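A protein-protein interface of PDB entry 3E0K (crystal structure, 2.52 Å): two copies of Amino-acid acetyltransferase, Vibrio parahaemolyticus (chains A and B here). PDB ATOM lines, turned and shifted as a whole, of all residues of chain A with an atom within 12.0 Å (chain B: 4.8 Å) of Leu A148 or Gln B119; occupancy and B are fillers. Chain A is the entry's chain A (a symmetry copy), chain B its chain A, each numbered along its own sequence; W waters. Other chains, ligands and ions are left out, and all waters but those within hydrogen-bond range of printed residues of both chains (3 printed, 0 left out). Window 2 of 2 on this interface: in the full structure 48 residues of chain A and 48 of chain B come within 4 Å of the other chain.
The side-chain carboxylate (OD1) of Asp A149 sits at hydrogen-bond distance from the side-chain hydroxyl (OH) of Tyr B122, at 2.8 Å.
N of Ala A147 lies within hydrogen-bond range of O of Tyr B122 (2.7 Å).
O of Ile B105 is in hydrogen-bond range of N of Leu A148 (2.7 Å).
N of Leu A150 lies within hydrogen-bond range of O of Asn B103 (2.9 Å).
The side-chain amide nitrogen of Gln B104 is in hydrogen-bond range of the side-chain carboxylate of Asp A149.
The side-chain amide nitrogen (NE2) of Gln B104 is in hydrogen-bond range of the side-chain hydroxyl (OH) of Tyr B122.
The backbone carbonyl oxygen of Phe B116 sits at hydrogen-bond distance from the backbone NH of Phe B121 (3.2 Å).
Among the printed residues, merely in contact across the chains: Ala A147 with Phe B121, Leu A148 with Gln B104, Leu A146 with Tyr B122, Ala A147 with Ile B105, Leu A148 with Gln B119, Leu A146 with Phe B116, Leu A148 with Gly B120, Leu A146 with Phe B121, Leu A148 with Phe B121, Leu A150 with Lys B94, Asp A149 with Asn B103, Leu A148 with Lys B94, Leu A146 with Ile B105, Leu A150 with Ile B105, Leu A150 with Gln B104, Ala A147 with Gly B120, Ile A145 with Tyr B122 and Leu A148 with Asn B103.
Of the printed residues of chain B, Ile A145 touches Tyr B122.
Printed residues of chain B within 4 Å of Leu A146: Ile B105, Phe B116, Phe B121 and Tyr B122.
Printed residues of chain B within 4 Å of Leu A148: Lys B94, Asn B103, Gln B104, Ile B105, Gln B119, Gly B120 and Phe B121.
Of chain A, only Leu A148 (3.9 Å) and Leu A150 (3.8 Å) come within 4 Å of Lys B94.
Of the printed residues of chain A, Asn B103 touches Leu A148, Asp A149 and Leu A150.
No residue of chain A comes within 4 Å of Trp B115.
Arg B117 touches none of the printed residues of chain A.
Of chain A, only Leu A148 (3.3 Å) comes within 4 Å of Gln B119.
Phe B121 touches three residues of chain A.
Printed residues of chain A within 4 Å of Tyr B122: Ile A145, Leu A146, Ala A147 and Asp A149.
The nearest printed residue of chain B that does not touch Ala A147 is Gln B104 (4.9 Å).
Printed residues of chain A that touch a printed residue of chain B: Ile A145, Leu A146, Ala A147, Leu A148, Asp A149 and Leu A150.
Hydrophobic or aromatic side chains of chain A within 4 Å of the printed part of chain B: Leu A146, Ala A147, Leu A148 and Leu A150.
Along chain A the printed residues that touch a printed residue of chain B span positions 145 to 150.
Printed residues of chain B that touch a printed residue of chain A: Lys B94, Asn B103, Gln B104, Ile B105, Phe B116, Gln B119, Gly B120, Phe B121 and Tyr B122.
Hydrophobic or aromatic side chains of chain B that line the printed part of chain A: Ile B105, Phe B116, Phe B121 and Tyr B122.
No position is printed for both chains.
Water W1 bridges O of Gly B120 (2.7 Å) and N of Asp A149 (2.7 Å).
Water W3 lies within hydrogen-bond range of the backbone carbonyl oxygen of Asp A149 (3.0 Å) and the side-chain amino group of Lys B94 (3.0 Å).
Water W2 lies within hydrogen-bond range of the side-chain carboxylate of Asp A149 (3.2 Å), the side-chain amide nitrogen of Gln B104 (3.3 Å) and the backbone carbonyl oxygen of Asn B103 (3.3 Å).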
ATOM      1  N   LYS A 144      -8.279 -15.647 -18.921  1.00  0.00           N
ATOM      2  CA  LYS A 144      -8.225 -14.450 -18.100  1.00  0.00           C
ATOM      3  C   LYS A 144      -8.123 -14.759 -16.616  1.00  0.00           C
ATOM      4  O   LYS A 144      -8.619 -15.796 -16.143  1.00  0.00           O
ATOM      5  CB  LYS A 144      -9.430 -13.570 -18.400  1.00  0.00           C
ATOM      6  CG  LYS A 144      -9.717 -13.449 -19.884  1.00  0.00           C
ATOM      7  CD  LYS A 144     -10.211 -12.060 -20.268  1.00  0.00           C
ATOM      8  CE  LYS A 144     -10.254 -11.870 -21.785  1.00  0.00           C
ATOM      9  NZ  LYS A 144      -8.949 -12.205 -22.411  1.00  0.00           N
ATOM     10  N   ILE A 145      -7.447 -13.873 -15.897  1.00  0.00           N
ATOM     11  CA  ILE A 145      -7.398 -13.907 -14.452  1.00  0.00           C
ATOM     12  C   ILE A 145      -8.350 -12.833 -13.921  1.00  0.00           C
ATOM     13  O   ILE A 145      -8.177 -11.650 -14.207  1.00  0.00           O
ATOM     14  CB  ILE A 145      -5.976 -13.599 -13.912  1.00  0.00           C
ATOM     15  CG1 ILE A 145      -4.920 -14.463 -14.605  1.00  0.00           C
ATOM     16  CG2 ILE A 145      -5.916 -13.773 -12.370  1.00  0.00           C
ATOM     17  CD1 ILE A 145      -3.492 -13.896 -14.496  1.00  0.00           C
ATOM     18  N   LEU A 146      -9.331 -13.236 -13.119  1.00  0.00           N
ATOM     19  CA  LEU A 146     -10.287 -12.275 -12.567  1.00  0.00           C
ATOM     20  C   LEU A 146     -10.244 -12.247 -11.036  1.00  0.00           C
ATOM     21  O   LEU A 146     -10.179 -13.308 -10.404  1.00  0.00           O
ATOM     22  CB  LEU A 146     -11.701 -12.583 -13.069  1.00  0.00           C
ATOM     23  CG  LEU A 146     -11.919 -12.726 -14.585  1.00  0.00           C
ATOM     24  CD1 LEU A 146     -13.374 -13.004 -14.843  1.00  0.00           C
ATOM     25  CD2 LEU A 146     -11.495 -11.490 -15.391  1.00  0.00           C
ATOM     26  N   ALA A 147     -10.263 -11.049 -10.452  1.00  0.00           N
ATOM     27  CA  ALA A 147     -10.247 -10.909  -8.999  1.00  0.00           C
ATOM     28  C   ALA A 147     -11.503 -10.240  -8.440  1.00  0.00           C
ATOM     29  O   ALA A 147     -12.143  -9.432  -9.112  1.00  0.00           O
ATOM     30  CB  ALA A 147      -8.996 -10.158  -8.540  1.00  0.00           C
ATOM     31  N   LEU A 148     -11.836 -10.582  -7.199  1.00  0.00           N
ATOM     32  CA  LEU A 148     -13.022 -10.057  -6.522  1.00  0.00           C
ATOM     33  C   LEU A 148     -12.637  -9.584  -5.121  1.00  0.00           C
ATOM     34  O   LEU A 148     -12.087 -10.358  -4.334  1.00  0.00           O
ATOM     35  CB  LEU A 148     -14.100 -11.138  -6.429  1.00  0.00           C
ATOM     36  CG  LEU A 148     -15.361 -10.809  -5.627  1.00  0.00           C
ATOM     37  CD1 LEU A 148     -16.209  -9.770  -6.356  1.00  0.00           C
ATOM     38  CD2 LEU A 148     -16.171 -12.077  -5.353  1.00  0.00           C
ATOM     39  N   ASP A 149     -12.911  -8.313  -4.832  1.00  0.00           N
ATOM     40  CA  ASP A 149     -12.718  -7.748  -3.502  1.00  0.00           C
ATOM     41  C   ASP A 149     -13.833  -8.193  -2.550  1.00  0.00           C
ATOM     42  O   ASP A 149     -15.027  -7.947  -2.791  1.00  0.00           O
ATOM     43  CB  ASP A 149     -12.665  -6.219  -3.584  1.00  0.00           C
ATOM     44  CG  ASP A 149     -11.456  -5.708  -4.375  1.00  0.00           C
ATOM     45  OD1 ASP A 149     -10.499  -6.478  -4.649  1.00  0.00           O
ATOM     46  OD2 ASP A 149     -11.455  -4.507  -4.719  1.00  0.00           O
ATOM     47  N   LEU A 150     -13.447  -8.863  -1.472  1.00  0.00           N
ATOM     48  CA  LEU A 150     -14.426  -9.367  -0.513  1.00  0.00           C
ATOM     49  C   LEU A 150     -14.731  -8.275   0.491  1.00  0.00           C
ATOM     50  O   LEU A 150     -14.128  -7.200   0.456  1.00  0.00           O
ATOM     51  CB  LEU A 150     -13.916 -10.620   0.208  1.00  0.00           C
ATOM     52  CG  LEU A 150     -13.428 -11.779  -0.665  1.00  0.00           C
ATOM     53  CD1 LEU A 150     -12.972 -12.933   0.173  1.00  0.00           C
ATOM     54  CD2 LEU A 150     -14.522 -12.211  -1.588  1.00  0.00           C
ATOM     55  OXT LEU A 150     -15.578  -8.445   1.375  1.00  0.00           O
ATOM     56  N   LEU B  87     -23.941 -18.885  -8.172  1.00  0.00           N
ATOM     57  CA  LEU B  87     -23.951 -17.753  -7.245  1.00  0.00           C
ATOM     58  C   LEU B  87     -23.948 -18.232  -5.780  1.00  0.00           C
ATOM     59  O   LEU B  87     -23.229 -17.704  -4.935  1.00  0.00           O
ATOM     60  CB  LEU B  87     -25.158 -16.848  -7.537  1.00  0.00           C
ATOM     61  CG  LEU B  87     -25.312 -15.524  -6.758  1.00  0.00           C
ATOM     62  CD1 LEU B  87     -24.012 -14.672  -6.705  1.00  0.00           C
ATOM     63  CD2 LEU B  87     -26.541 -14.681  -7.255  1.00  0.00           C
ATOM     64  N   LEU B  90     -20.490 -19.250  -4.946  1.00  0.00           N
ATOM     65  CA  LEU B  90     -19.613 -18.100  -4.835  1.00  0.00           C
ATOM     66  C   LEU B  90     -19.832 -17.380  -3.506  1.00  0.00           C
ATOM     67  O   LEU B  90     -18.873 -17.097  -2.792  1.00  0.00           O
ATOM     68  CB  LEU B  90     -19.767 -17.151  -6.033  1.00  0.00           C
ATOM     69  CG  LEU B  90     -19.160 -15.760  -5.892  1.00  0.00           C
ATOM     70  CD1 LEU B  90     -17.669 -15.830  -5.685  1.00  0.00           C
ATOM     71  CD2 LEU B  90     -19.498 -14.915  -7.100  1.00  0.00           C
ATOM     72  N   LYS B  94     -17.162 -16.639  -0.783  1.00  0.00           N
ATOM     73  CA  LYS B  94     -16.915 -15.301  -0.275  1.00  0.00           C
ATOM     74  C   LYS B  94     -16.955 -15.317   1.252  1.00  0.00           C
ATOM     75  O   LYS B  94     -15.988 -14.937   1.901  1.00  0.00           O
ATOM     76  CB  LYS B  94     -17.941 -14.303  -0.821  1.00  0.00           C
ATOM     77  CG  LYS B  94     -17.786 -13.977  -2.301  1.00  0.00           C
ATOM     78  CD  LYS B  94     -18.911 -13.090  -2.812  1.00  0.00           C
ATOM     79  CE  LYS B  94     -18.765 -11.685  -2.281  1.00  0.00           C
ATOM     80  NZ  LYS B  94     -19.813 -10.836  -2.830  1.00  0.00           N
ATOM     81  N   ASN B 103      -9.069 -11.580   1.715  1.00  0.00           N
ATOM     82  CA  ASN B 103      -9.877 -10.447   1.261  1.00  0.00           C
ATOM     83  C   ASN B 103     -10.059 -10.362  -0.247  1.00  0.00           C
ATOM     84  O   ASN B 103     -10.653  -9.389  -0.729  1.00  0.00           O
ATOM     85  CB  ASN B 103      -9.358  -9.110   1.824  1.00  0.00           C
ATOM     86  CG  ASN B 103      -7.929  -8.795   1.384  1.00  0.00           C
ATOM     87  OD1 ASN B 103      -7.514  -9.161   0.284  1.00  0.00           O
ATOM     88  ND2 ASN B 103      -7.172  -8.123   2.245  1.00  0.00           N
ATOM     89  N   GLN B 104      -9.547 -11.362  -0.976  1.00  0.00           N
ATOM     90  CA  GLN B 104      -9.768 -11.471  -2.423  1.00  0.00           C
ATOM     91  C   GLN B 104      -9.898 -12.889  -2.907  1.00  0.00           C
ATOM     92  O   GLN B 104      -9.180 -13.761  -2.449  1.00  0.00           O
ATOM     93  CB  GLN B 104      -8.642 -10.818  -3.200  1.00  0.00           C
ATOM     94  CG  GLN B 104      -8.798  -9.343  -3.277  1.00  0.00           C
ATOM     95  CD  GLN B 104      -7.622  -8.673  -3.923  1.00  0.00           C
ATOM     96  OE1 GLN B 104      -6.637  -9.322  -4.288  1.00  0.00           O
ATOM     97  NE2 GLN B 104      -7.714  -7.352  -4.076  1.00  0.00           N
ATOM     98  N   ILE B 105     -10.830 -13.103  -3.837  1.00  0.00           N
ATOM     99  CA  ILE B 105     -10.944 -14.355  -4.583  1.00  0.00           C
ATOM    100  C   ILE B 105     -10.556 -14.083  -6.035  1.00  0.00           C
ATOM    101  O   ILE B 105     -10.908 -13.032  -6.596  1.00  0.00           O
ATOM    102  CB  ILE B 105     -12.371 -14.939  -4.524  1.00  0.00           C
ATOM    103  CG1 ILE B 105     -12.707 -15.336  -3.083  1.00  0.00           C
ATOM    104  CG2 ILE B 105     -12.531 -16.145  -5.481  1.00  0.00           C
ATOM    105  CD1 ILE B 105     -13.914 -16.249  -2.955  1.00  0.00           C
ATOM    106  N   TRP B 115     -20.893 -12.880 -16.558  1.00  0.00           N
ATOM    107  CA  TRP B 115     -21.320 -13.301 -15.222  1.00  0.00           C
ATOM    108  C   TRP B 115     -20.347 -12.884 -14.132  1.00  0.00           C
ATOM    109  O   TRP B 115     -20.748 -12.381 -13.078  1.00  0.00           O
ATOM    110  CB  TRP B 115     -21.497 -14.812 -15.162  1.00  0.00           C
ATOM    111  CG  TRP B 115     -22.146 -15.283 -13.875  1.00  0.00           C
ATOM    112  CD1 TRP B 115     -23.488 -15.304 -13.595  1.00  0.00           C
ATOM    113  CD2 TRP B 115     -21.489 -15.798 -12.707  1.00  0.00           C
ATOM    114  NE1 TRP B 115     -23.701 -15.805 -12.335  1.00  0.00           N
ATOM    115  CE2 TRP B 115     -22.497 -16.118 -11.766  1.00  0.00           C
ATOM    116  CE3 TRP B 115     -20.152 -16.018 -12.365  1.00  0.00           C
ATOM    117  CZ2 TRP B 115     -22.214 -16.651 -10.513  1.00  0.00           C
ATOM    118  CZ3 TRP B 115     -19.868 -16.544 -11.112  1.00  0.00           C
ATOM    119  CH2 TRP B 115     -20.900 -16.855 -10.200  1.00  0.00           C
ATOM    120  N   PHE B 116     -19.067 -13.117 -14.381  1.00  0.00           N
ATOM    121  CA  PHE B 116     -18.050 -12.727 -13.429  1.00  0.00           C
ATOM    122  C   PHE B 116     -18.033 -11.224 -13.212  1.00  0.00           C
ATOM    123  O   PHE B 116     -18.048 -10.776 -12.064  1.00  0.00           O
ATOM    124  CB  PHE B 116     -16.682 -13.263 -13.827  1.00  0.00           C
ATOM    125  CG  PHE B 116     -16.477 -14.713 -13.482  1.00  0.00           C
ATOM    126  CD1 PHE B 116     -16.342 -15.120 -12.156  1.00  0.00           C
ATOM    127  CD2 PHE B 116     -16.402 -15.680 -14.485  1.00  0.00           C
ATOM    128  CE1 PHE B 116     -16.145 -16.473 -11.837  1.00  0.00           C
ATOM    129  CE2 PHE B 116     -16.198 -17.038 -14.168  1.00  0.00           C
ATOM    130  CZ  PHE B 116     -16.071 -17.425 -12.848  1.00  0.00           C
ATOM    131  N   ARG B 117     -18.035 -10.453 -14.299  1.00  0.00           N
ATOM    132  CA  ARG B 117     -18.092  -8.991 -14.200  1.00  0.00           C
ATOM    133  C   ARG B 117     -19.311  -8.566 -13.378  1.00  0.00           C
ATOM    134  O   ARG B 117     -19.217  -7.706 -12.493  1.00  0.00           O
ATOM    135  CB  ARG B 117     -18.090  -8.330 -15.589  1.00  0.00           C
ATOM    136  CG  ARG B 117     -18.342  -6.784 -15.582  1.00  0.00           C
ATOM    137  CD  ARG B 117     -17.661  -6.036 -16.766  1.00  0.00           C
ATOM    138  NE  ARG B 117     -16.219  -6.324 -16.800  1.00  0.00           N
ATOM    139  CZ  ARG B 117     -15.610  -7.088 -17.715  1.00  0.00           C
ATOM    140  NH1 ARG B 117     -16.315  -7.631 -18.707  1.00  0.00           N
ATOM    141  NH2 ARG B 117     -14.291  -7.302 -17.649  1.00  0.00           N
ATOM    142  N   GLU B 118     -20.445  -9.201 -13.660  1.00  0.00           N
ATOM    143  CA  GLU B 118     -21.669  -8.942 -12.926  1.00  0.00           C
ATOM    144  C   GLU B 118     -21.543  -9.188 -11.430  1.00  0.00           C
ATOM    145  O   GLU B 118     -22.300  -8.604 -10.660  1.00  0.00           O
ATOM    146  CB  GLU B 118     -22.834  -9.753 -13.484  1.00  0.00           C
ATOM    147  CG  GLU B 118     -23.519  -9.094 -14.666  1.00  0.00           C
ATOM    148  CD  GLU B 118     -24.642  -9.964 -15.234  1.00  0.00           C
ATOM    149  OE1 GLU B 118     -24.366 -11.115 -15.676  1.00  0.00           O
ATOM    150  OE2 GLU B 118     -25.810  -9.492 -15.235  1.00  0.00           O
ATOM    151  N   GLN B 119     -20.610 -10.042 -11.010  1.00  0.00           N
ATOM    152  CA  GLN B 119     -20.429 -10.255  -9.573  1.00  0.00           C
ATOM    153  C   GLN B 119     -19.403  -9.317  -8.936  1.00  0.00           C
ATOM    154  O   GLN B 119     -19.229  -9.333  -7.715  1.00  0.00           O
ATOM    155  CB  GLN B 119     -20.119 -11.710  -9.240  1.00  0.00           C
ATOM    156  CG  GLN B 119     -21.035 -12.718  -9.890  1.00  0.00           C
ATOM    157  CD  GLN B 119     -22.504 -12.466  -9.626  1.00  0.00           C
ATOM    158  OE1 GLN B 119     -23.326 -12.654 -10.518  1.00  0.00           O
ATOM    159  NE2 GLN B 119     -22.847 -12.045  -8.400  1.00  0.00           N
ATOM    160  N   GLY B 120     -18.758  -8.488  -9.756  1.00  0.00           N
ATOM    161  CA  GLY B 120     -17.816  -7.490  -9.269  1.00  0.00           C
ATOM    162  C   GLY B 120     -16.375  -7.931  -9.452  1.00  0.00           C
ATOM    163  O   GLY B 120     -15.457  -7.295  -8.926  1.00  0.00           O
ATOM    164  N   PHE B 121     -16.175  -9.023 -10.186  1.00  0.00           N
ATOM    165  CA  PHE B 121     -14.837  -9.458 -10.597  1.00  0.00           C
ATOM    166  C   PHE B 121     -14.246  -8.477 -11.609  1.00  0.00           C
ATOM    167  O   PHE B 121     -14.969  -7.968 -12.467  1.00  0.00           O
ATOM    168  CB  PHE B 121     -14.897 -10.844 -11.258  1.00  0.00           C
ATOM    169  CG  PHE B 121     -14.921 -12.006 -10.284  1.00  0.00           C
ATOM    170  CD1 PHE B 121     -13.746 -12.670  -9.939  1.00  0.00           C
ATOM    171  CD2 PHE B 121     -16.118 -12.451  -9.737  1.00  0.00           C
ATOM    172  CE1 PHE B 121     -13.772 -13.741  -9.063  1.00  0.00           C
ATOM    173  CE2 PHE B 121     -16.139 -13.525  -8.848  1.00  0.00           C
ATOM    174  CZ  PHE B 121     -14.969 -14.168  -8.518  1.00  0.00           C
ATOM    175  N   TYR B 122     -12.940  -8.229 -11.513  1.00  0.00           N
ATOM    176  CA  TYR B 122     -12.236  -7.406 -12.489  1.00  0.00           C
ATOM    177  C   TYR B 122     -10.985  -8.154 -12.972  1.00  0.00           C
ATOM    178  O   TYR B 122     -10.471  -9.041 -12.279  1.00  0.00           O
ATOM    179  CB  TYR B 122     -11.892  -5.999 -11.935  1.00  0.00           C
ATOM    180  CG  TYR B 122     -11.108  -6.043 -10.646  1.00  0.00           C
ATOM    181  CD1 TYR B 122      -9.702  -6.005 -10.638  1.00  0.00           C
ATOM    182  CD2 TYR B 122     -11.773  -6.162  -9.419  1.00  0.00           C
ATOM    183  CE1 TYR B 122      -8.988  -6.068  -9.438  1.00  0.00           C
ATOM    184  CE2 TYR B 122     -11.069  -6.238  -8.212  1.00  0.00           C
ATOM    185  CZ  TYR B 122      -9.681  -6.182  -8.222  1.00  0.00           C
ATOM    186  OH  TYR B 122      -9.025  -6.244  -6.996  1.00  0.00           O
HETATM  187  O   HOH W   1     -14.083  -6.724  -6.683  1.00  0.00           O
HETATM  188  O   HOH W   2      -9.615  -6.402  -1.588  1.00  0.00           O
HETATM  189  O   HOH W   3     -18.023  -8.369  -2.741  1.00  0.00           O
